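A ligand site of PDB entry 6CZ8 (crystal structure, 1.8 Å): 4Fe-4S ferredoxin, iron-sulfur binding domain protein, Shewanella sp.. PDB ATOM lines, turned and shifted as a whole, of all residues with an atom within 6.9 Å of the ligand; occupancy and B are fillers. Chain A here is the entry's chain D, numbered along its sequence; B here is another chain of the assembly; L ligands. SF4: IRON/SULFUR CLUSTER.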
ATOM      1  N   ILE A   7     -19.520   0.285   1.947  1.00  0.00           N
ATOM      2  CA  ILE A   7     -18.842  -0.016   3.210  1.00  0.00           C
ATOM      3  C   ILE A   7     -18.434   1.300   3.842  1.00  0.00           C
ATOM      4  O   ILE A   7     -17.746   2.124   3.208  1.00  0.00           O
ATOM      5  CB  ILE A   7     -17.628  -0.927   2.991  1.00  0.00           C
ATOM      6  CG1 ILE A   7     -18.070  -2.282   2.411  1.00  0.00           C
ATOM      7  CG2 ILE A   7     -16.881  -1.115   4.306  1.00  0.00           C
ATOM      8  CD1 ILE A   7     -16.955  -3.193   2.064  1.00  0.00           C
ATOM      9  N   ASP A   8     -18.844   1.506   5.088  1.00  0.00           N
ATOM     10  CA  ASP A   8     -18.572   2.731   5.834  1.00  0.00           C
ATOM     11  C   ASP A   8     -17.308   2.510   6.657  1.00  0.00           C
ATOM     12  O   ASP A   8     -17.322   1.767   7.646  1.00  0.00           O
ATOM     13  CB  ASP A   8     -19.763   3.079   6.720  1.00  0.00           C
ATOM     14  CG  ASP A   8     -19.587   4.384   7.465  1.00  0.00           C
ATOM     15  OD1 ASP A   8     -18.437   4.742   7.807  1.00  0.00           O
ATOM     16  OD2 ASP A   8     -20.612   5.078   7.718  1.00  0.00           O
ATOM     17  N   LYS A  11     -17.240   3.367  10.435  1.00  0.00           N
ATOM     18  CA  LYS A  11     -17.864   2.345  11.274  1.00  0.00           C
ATOM     19  C   LYS A  11     -17.010   1.091  11.383  1.00  0.00           C
ATOM     20  O   LYS A  11     -17.034   0.405  12.411  1.00  0.00           O
ATOM     21  CB  LYS A  11     -19.244   1.980  10.740  1.00  0.00           C
ATOM     22  CG  LYS A  11     -20.312   3.055  10.929  1.00  0.00           C
ATOM     23  CD  LYS A  11     -21.606   2.614  10.218  1.00  0.00           C
ATOM     24  CE  LYS A  11     -22.815   3.503  10.632  1.00  0.00           C
ATOM     25  NZ  LYS A  11     -23.363   3.032  11.946  1.00  0.00           N
ATOM     26  N   CYS A  12     -16.234   0.779  10.343  1.00  0.00           N
ATOM     27  CA  CYS A  12     -15.425  -0.440  10.321  1.00  0.00           C
ATOM     28  C   CYS A  12     -14.346  -0.382  11.385  1.00  0.00           C
ATOM     29  O   CYS A  12     -13.620   0.631  11.490  1.00  0.00           O
ATOM     30  CB  CYS A  12     -14.778  -0.617   8.945  1.00  0.00           C
ATOM     31  SG  CYS A  12     -13.757  -2.090   8.784  1.00  0.00           S
ATOM     32  N   VAL A  13     -14.190  -1.481  12.150  1.00  0.00           N
ATOM     33  CA  VAL A  13     -13.165  -1.544  13.189  1.00  0.00           C
ATOM     34  C   VAL A  13     -12.018  -2.467  12.784  1.00  0.00           C
ATOM     35  O   VAL A  13     -11.119  -2.716  13.584  1.00  0.00           O
ATOM     36  CB  VAL A  13     -13.743  -1.952  14.566  1.00  0.00           C
ATOM     37  CG1 VAL A  13     -14.742  -0.881  15.038  1.00  0.00           C
ATOM     38  CG2 VAL A  13     -14.388  -3.346  14.546  1.00  0.00           C
ATOM     39  N   GLY A  14     -12.030  -2.984  11.565  1.00  0.00           N
ATOM     40  CA  GLY A  14     -10.922  -3.758  11.041  1.00  0.00           C
ATOM     41  C   GLY A  14     -10.737  -5.096  11.721  1.00  0.00           C
ATOM     42  O   GLY A  14      -9.594  -5.562  11.843  1.00  0.00           O
ATOM     43  N   CYS A  15     -11.833  -5.746  12.100  1.00  0.00           N
ATOM     44  CA  CYS A  15     -11.783  -6.958  12.924  1.00  0.00           C
ATOM     45  C   CYS A  15     -11.734  -8.260  12.132  1.00  0.00           C
ATOM     46  O   CYS A  15     -11.416  -9.289  12.718  1.00  0.00           O
ATOM     47  CB  CYS A  15     -13.008  -6.995  13.854  1.00  0.00           C
ATOM     48  SG  CYS A  15     -14.660  -7.163  13.041  1.00  0.00           S
ATOM     49  N   GLY A  16     -12.090  -8.266  10.853  1.00  0.00           N
ATOM     50  CA  GLY A  16     -12.088  -9.481  10.075  1.00  0.00           C
ATOM     51  C   GLY A  16     -13.285 -10.370  10.287  1.00  0.00           C
ATOM     52  O   GLY A  16     -13.307 -11.512   9.775  1.00  0.00           O
ATOM     53  N   GLY A  17     -14.295  -9.899  11.024  1.00  0.00           N
ATOM     54  CA  GLY A  17     -15.472 -10.735  11.267  1.00  0.00           C
ATOM     55  C   GLY A  17     -16.194 -11.122   9.995  1.00  0.00           C
ATOM     56  O   GLY A  17     -16.727 -12.217   9.872  1.00  0.00           O
ATOM     57  N   CYS A  18     -16.246 -10.204   9.038  1.00  0.00           N
ATOM     58  CA  CYS A  18     -16.824 -10.478   7.728  1.00  0.00           C
ATOM     59  C   CYS A  18     -16.102 -11.598   7.026  1.00  0.00           C
ATOM     60  O   CYS A  18     -16.734 -12.464   6.403  1.00  0.00           O
ATOM     61  CB  CYS A  18     -16.795  -9.195   6.892  1.00  0.00           C
ATOM     62  SG  CYS A  18     -15.166  -8.327   7.016  1.00  0.00           S
ATOM     63  N   SER A  19     -14.766 -11.589   7.059  1.00  0.00           N
ATOM     64  CA  SER A  19     -14.004 -12.618   6.371  1.00  0.00           C
ATOM     65  C   SER A  19     -14.175 -13.982   7.057  1.00  0.00           C
ATOM     66  O   SER A  19     -14.261 -15.009   6.384  1.00  0.00           O
ATOM     67  CB  SER A  19     -12.536 -12.210   6.303  1.00  0.00           C
ATOM     68  OG  SER A  19     -12.396 -10.965   5.624  1.00  0.00           O
ATOM     69  N   SER A  35     -13.574 -13.099   1.090  1.00  0.00           N
ATOM     70  CA  SER A  35     -13.497 -11.840   1.810  1.00  0.00           C
ATOM     71  C   SER A  35     -12.117 -11.745   2.441  1.00  0.00           C
ATOM     72  O   SER A  35     -11.649 -12.692   3.062  1.00  0.00           O
ATOM     73  CB  SER A  35     -14.567 -11.786   2.905  1.00  0.00           C
ATOM     74  OG  SER A  35     -14.357 -10.663   3.752  1.00  0.00           O
ATOM     75  N   HIS A  37      -8.798  -8.372   3.204  1.00  0.00           N
ATOM     76  CA  HIS A  37      -8.593  -6.976   3.567  1.00  0.00           C
ATOM     77  C   HIS A  37      -7.281  -6.509   2.980  1.00  0.00           C
ATOM     78  O   HIS A  37      -6.444  -7.321   2.574  1.00  0.00           O
ATOM     79  CB  HIS A  37      -8.566  -6.800   5.085  1.00  0.00           C
ATOM     80  CG  HIS A  37      -7.497  -7.607   5.739  1.00  0.00           C
ATOM     81  ND1 HIS A  37      -7.739  -8.855   6.269  1.00  0.00           N
ATOM     82  CD2 HIS A  37      -6.168  -7.370   5.930  1.00  0.00           C
ATOM     83  CE1 HIS A  37      -6.616  -9.357   6.751  1.00  0.00           C
ATOM     84  NE2 HIS A  37      -5.654  -8.472   6.556  1.00  0.00           N
ATOM     85  N   TYR A  52      -7.448   0.159   7.423  1.00  0.00           N
ATOM     86  CA  TYR A  52      -7.922  -1.171   7.059  1.00  0.00           C
ATOM     87  C   TYR A  52      -9.066  -1.017   6.072  1.00  0.00           C
ATOM     88  O   TYR A  52     -10.004  -0.242   6.306  1.00  0.00           O
ATOM     89  CB  TYR A  52      -8.366  -1.943   8.325  1.00  0.00           C
ATOM     90  CG  TYR A  52      -8.923  -3.339   8.147  1.00  0.00           C
ATOM     91  CD1 TYR A  52     -10.179  -3.542   7.622  1.00  0.00           C
ATOM     92  CD2 TYR A  52      -8.208  -4.449   8.584  1.00  0.00           C
ATOM     93  CE1 TYR A  52     -10.701  -4.811   7.494  1.00  0.00           C
ATOM     94  CE2 TYR A  52      -8.716  -5.709   8.458  1.00  0.00           C
ATOM     95  CZ  TYR A  52      -9.963  -5.892   7.938  1.00  0.00           C
ATOM     96  OH  TYR A  52     -10.472  -7.162   7.812  1.00  0.00           O
ATOM     97  N   PRO A  54     -11.729  -3.488   4.030  1.00  0.00           N
ATOM     98  CA  PRO A  54     -12.227  -4.839   3.709  1.00  0.00           C
ATOM     99  C   PRO A  54     -12.392  -4.978   2.211  1.00  0.00           C
ATOM    100  O   PRO A  54     -12.822  -4.043   1.540  1.00  0.00           O
ATOM    101  CB  PRO A  54     -13.592  -4.918   4.410  1.00  0.00           C
ATOM    102  CG  PRO A  54     -13.659  -3.700   5.308  1.00  0.00           C
ATOM    103  CD  PRO A  54     -12.764  -2.661   4.682  1.00  0.00           C
ATOM    104  N   CYS A 179     -21.412 -11.802   5.405  1.00  0.00           N
ATOM    105  CA  CYS A 179     -20.551 -10.751   5.914  1.00  0.00           C
ATOM    106  C   CYS A 179     -21.348  -9.556   6.394  1.00  0.00           C
ATOM    107  O   CYS A 179     -20.912  -8.862   7.302  1.00  0.00           O
ATOM    108  CB  CYS A 179     -19.529 -10.327   4.861  1.00  0.00           C
ATOM    109  SG  CYS A 179     -20.282  -9.883   3.283  1.00  0.00           S
ATOM    110  N   ALA A 182     -22.669 -10.291   9.783  1.00  0.00           N
ATOM    111  CA  ALA A 182     -21.586 -10.495  10.732  1.00  0.00           C
ATOM    112  C   ALA A 182     -20.957  -9.191  11.222  1.00  0.00           C
ATOM    113  O   ALA A 182     -20.174  -9.235  12.170  1.00  0.00           O
ATOM    114  CB  ALA A 182     -20.492 -11.345  10.101  1.00  0.00           C
ATOM    115  N   CYS A 183     -21.258  -8.071  10.580  1.00  0.00           N
ATOM    116  CA  CYS A 183     -20.566  -6.823  10.873  1.00  0.00           C
ATOM    117  C   CYS A 183     -21.203  -6.134  12.078  1.00  0.00           C
ATOM    118  O   CYS A 183     -22.400  -5.823  12.030  1.00  0.00           O
ATOM    119  CB  CYS A 183     -20.612  -5.900   9.691  1.00  0.00           C
ATOM    120  SG  CYS A 183     -19.706  -4.377  10.056  1.00  0.00           S
ATOM    121  N   PRO A 184     -20.451  -5.909  13.172  1.00  0.00           N
ATOM    122  CA  PRO A 184     -21.093  -5.417  14.409  1.00  0.00           C
ATOM    123  C   PRO A 184     -21.633  -4.022  14.290  1.00  0.00           C
ATOM    124  O   PRO A 184     -22.584  -3.681  15.009  1.00  0.00           O
ATOM    125  CB  PRO A 184     -19.962  -5.501  15.448  1.00  0.00           C
ATOM    126  CG  PRO A 184     -18.705  -5.430  14.627  1.00  0.00           C
ATOM    127  CD  PRO A 184     -19.028  -6.220  13.355  1.00  0.00           C
ATOM    128  N   SER A 185     -21.043  -3.206  13.406  1.00  0.00           N
ATOM    129  CA  SER A 185     -21.448  -1.819  13.254  1.00  0.00           C
ATOM    130  C   SER A 185     -22.341  -1.592  12.037  1.00  0.00           C
ATOM    131  O   SER A 185     -22.640  -0.425  11.708  1.00  0.00           O
ATOM    132  CB  SER A 185     -20.219  -0.944  13.167  1.00  0.00           C
ATOM    133  OG  SER A 185     -19.399  -1.396  12.108  1.00  0.00           O
ATOM    134  N   GLU A 186     -22.793  -2.664  11.379  1.00  0.00           N
ATOM    135  CA  GLU A 186     -23.610  -2.543  10.179  1.00  0.00           C
ATOM    136  C   GLU A 186     -22.914  -1.658   9.143  1.00  0.00           C
ATOM    137  O   GLU A 186     -23.545  -0.837   8.463  1.00  0.00           O
ATOM    138  CB  GLU A 186     -25.015  -2.003  10.514  1.00  0.00           C
ATOM    139  CG  GLU A 186     -25.843  -2.917  11.401  1.00  0.00           C
ATOM    140  CD  GLU A 186     -27.185  -2.297  11.770  1.00  0.00           C
ATOM    141  OE1 GLU A 186     -27.389  -1.102  11.483  1.00  0.00           O
ATOM    142  OE2 GLU A 186     -28.027  -3.014  12.344  1.00  0.00           O
ATOM    143  N   ALA A 187     -21.603  -1.834   9.014  1.00  0.00           N
ATOM    144  CA  ALA A 187     -20.840  -0.987   8.105  1.00  0.00           C
ATOM    145  C   ALA A 187     -21.078  -1.346   6.652  1.00  0.00           C
ATOM    146  O   ALA A 187     -20.799  -0.519   5.777  1.00  0.00           O
ATOM    147  CB  ALA A 187     -19.352  -1.078   8.445  1.00  0.00           C
ATOM    148  N   ARG A 188     -21.585  -2.556   6.386  1.00  0.00           N
ATOM    149  CA  ARG A 188     -21.751  -3.070   5.030  1.00  0.00           C
ATOM    150  C   ARG A 188     -23.235  -3.051   4.682  1.00  0.00           C
ATOM    151  O   ARG A 188     -24.048  -3.603   5.430  1.00  0.00           O
ATOM    152  CB  ARG A 188     -21.191  -4.501   4.919  1.00  0.00           C
ATOM    153  CG  ARG A 188     -19.756  -4.630   5.445  1.00  0.00           C
ATOM    154  CD  ARG A 188     -19.380  -6.066   5.731  1.00  0.00           C
ATOM    155  NE  ARG A 188     -19.091  -6.863   4.533  1.00  0.00           N
ATOM    156  CZ  ARG A 188     -17.887  -7.019   3.988  1.00  0.00           C
ATOM    157  NH1 ARG A 188     -16.825  -6.403   4.504  1.00  0.00           N
ATOM    158  NH2 ARG A 188     -17.726  -7.776   2.913  1.00  0.00           N
ATOM    159  N   PHE A 228     -11.275   5.445   7.717  1.00  0.00           N
ATOM    160  CA  PHE A 228     -11.033   4.569   8.868  1.00  0.00           C
ATOM    161  C   PHE A 228     -10.581   5.368  10.074  1.00  0.00           C
ATOM    162  O   PHE A 228     -11.015   5.113  11.204  1.00  0.00           O
ATOM    163  CB  PHE A 228     -10.011   3.507   8.464  1.00  0.00           C
ATOM    164  CG  PHE A 228      -9.830   2.414   9.481  1.00  0.00           C
ATOM    165  CD1 PHE A 228     -10.667   1.314   9.472  1.00  0.00           C
ATOM    166  CD2 PHE A 228      -8.838   2.482  10.433  1.00  0.00           C
ATOM    167  CE1 PHE A 228     -10.512   0.300  10.390  1.00  0.00           C
ATOM    168  CE2 PHE A 228      -8.661   1.466  11.348  1.00  0.00           C
ATOM    169  CZ  PHE A 228      -9.512   0.367  11.337  1.00  0.00           C
ATOM    170  N   SER B  55     -21.526  -8.570  16.943  1.00  0.00           N
ATOM    171  CA  SER B  55     -20.531  -9.503  17.451  1.00  0.00           C
ATOM    172  C   SER B  55     -19.112  -9.091  17.039  1.00  0.00           C
ATOM    173  O   SER B  55     -18.887  -8.520  15.979  1.00  0.00           O
ATOM    174  CB  SER B  55     -20.764 -10.916  16.890  1.00  0.00           C
ATOM    175  OG  SER B  55     -19.799 -11.813  17.416  1.00  0.00           O
ATOM    176  N   PRO B  57     -15.229 -10.689  16.043  1.00  0.00           N
ATOM    177  CA  PRO B  57     -14.956 -11.730  15.036  1.00  0.00           C
ATOM    178  C   PRO B  57     -14.768 -13.115  15.607  1.00  0.00           C
ATOM    179  O   PRO B  57     -14.867 -14.084  14.842  1.00  0.00           O
ATOM    180  CB  PRO B  57     -13.660 -11.237  14.347  1.00  0.00           C
ATOM    181  CG  PRO B  57     -12.955 -10.439  15.439  1.00  0.00           C
ATOM    182  CD  PRO B  57     -14.102  -9.744  16.217  1.00  0.00           C
ATOM    183  N   SER B 199     -17.662  -2.230  19.606  1.00  0.00           N
ATOM    184  CA  SER B 199     -17.420  -2.208  18.153  1.00  0.00           C
ATOM    185  C   SER B 199     -18.631  -1.669  17.387  1.00  0.00           C
ATOM    186  O   SER B 199     -18.498  -1.016  16.348  1.00  0.00           O
ATOM    187  CB  SER B 199     -17.065  -3.619  17.645  1.00  0.00           C
ATOM    188  OG  SER B 199     -15.837  -4.080  18.196  1.00  0.00           O
ATOM    189  N   ARG B 686      -6.775  -9.879  19.099  1.00  0.00           N
ATOM    190  CA  ARG B 686      -8.218  -9.698  18.978  1.00  0.00           C
ATOM    191  C   ARG B 686      -8.892 -10.975  18.504  1.00  0.00           C
ATOM    192  O   ARG B 686     -10.136 -11.013  18.470  1.00  0.00           O
ATOM    193  CB  ARG B 686      -8.536  -8.504  18.073  1.00  0.00           C
ATOM    194  CG  ARG B 686      -8.530  -8.749  16.587  1.00  0.00           C
ATOM    195  CD  ARG B 686      -8.448  -7.435  15.784  1.00  0.00           C
ATOM    196  NE  ARG B 686      -9.546  -6.503  16.080  1.00  0.00           N
ATOM    197  CZ  ARG B 686      -9.660  -5.281  15.556  1.00  0.00           C
ATOM    198  NH1 ARG B 686      -8.752  -4.838  14.690  1.00  0.00           N
ATOM    199  NH2 ARG B 686     -10.689  -4.508  15.854  1.00  0.00           N
ATOM    200  N   VAL B 705      -5.227  -9.244  11.479  1.00  0.00           N
ATOM    201  CA  VAL B 705      -6.208  -8.243  11.908  1.00  0.00           C
ATOM    202  C   VAL B 705      -5.748  -7.535  13.189  1.00  0.00           C
ATOM    203  O   VAL B 705      -6.245  -6.447  13.493  1.00  0.00           O
ATOM    204  CB  VAL B 705      -7.613  -8.841  12.107  1.00  0.00           C
ATOM    205  CG1 VAL B 705      -8.141  -9.349  10.758  1.00  0.00           C
ATOM    206  CG2 VAL B 705      -7.679  -9.901  13.183  1.00  0.00           C
HETATM  207 FE1  SF4 L   1     -15.287  -5.958  11.067  1.00  0.00          FE
HETATM  208 FE2  SF4 L   1     -15.061  -3.936   9.189  1.00  0.00          FE
HETATM  209 FE3  SF4 L   1     -17.483  -4.986   9.718  1.00  0.00          FE
HETATM  210 FE4  SF4 L   1     -15.653  -6.475   8.409  1.00  0.00          FE
HETATM  211  S1  SF4 L   1     -16.589  -4.531   7.639  1.00  0.00           S
HETATM  212  S2  SF4 L   1     -16.982  -7.163  10.151  1.00  0.00           S
HETATM  213  S3  SF4 L   1     -13.697  -5.722   9.390  1.00  0.00           S
HETATM  214  S4  SF4 L   1     -16.181  -3.893  11.260  1.00  0.00           S
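SG of Cys 12 sits close to N of Gly 14 (3.4 Å). The side-chain hydroxyl (OG) of Ser 185 sits close to the side-chain sulfur (SG) of Cys 183, at 3.6 Å. The side-chain sulfur (SG) of Cys 183 sits close to the backbone NH (N) of Ala 187 (3.3 Å). The backbone NH (N) of Glu 186 sits close to the side-chain sulfur (SG) of Cys 183 (3.8 Å). SG of Cys 18 lies close to NH1 of Arg 188 (3.6 Å). The backbone carbonyl oxygen of Val 13 lies within hydrogen-bond range of the guanidinium group of Arg 686 of chain B, at 2.9 Å. The guanidinium group of Arg 188 lies close to the side-chain sulfur of Cys 179, at 3.3 Å. NH1 of Arg 686 of chain B lies within hydrogen-bond range of O of Gly 14, at 3.1 Å.
Merely in contact with the ligand: Gly 14 (3.8 Å), Gly 17 (3.9 Å), Tyr 52 (3.7 Å), Pro 54 (3.8 Å) and Pro 184 (3.9 Å). 12 residues have an atom within 4 Å of the ligand: Cys 12, Val 13, Gly 14, Cys 15, Gly 16, Gly 17, Cys 18, Tyr 52, Pro 54, Cys 183, Pro 184 and Arg 188.
The side-chain sulfur (SG) of Cys 12 is bound to an iron atom (FE2) of the ligand. FE3 of the ligand is bound by SG of Cys 183, 2.3 Å away. The backbone NH (N) of Cys 18 sits close to a sulfur (S2) of the ligand. The side-chain sulfur of Cys 18 binds an iron atom (FE4) of the ligand (2.4 Å). S3 of the ligand lies close to N of Cys 15 (3.3 Å). SG of Cys 15 binds FE1 of the ligand, 2.4 Å away. The backbone NH of Val 13 lies close to a sulfur (S4) of the ligand, at 3.3 Å. The backbone NH of Gly 16 lies close to a sulfur (S3) of the ligand (3.3 Å). A sulfur (S1) of the ligand lies close to the guanidinium group of Arg 188 (3.7 Å).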
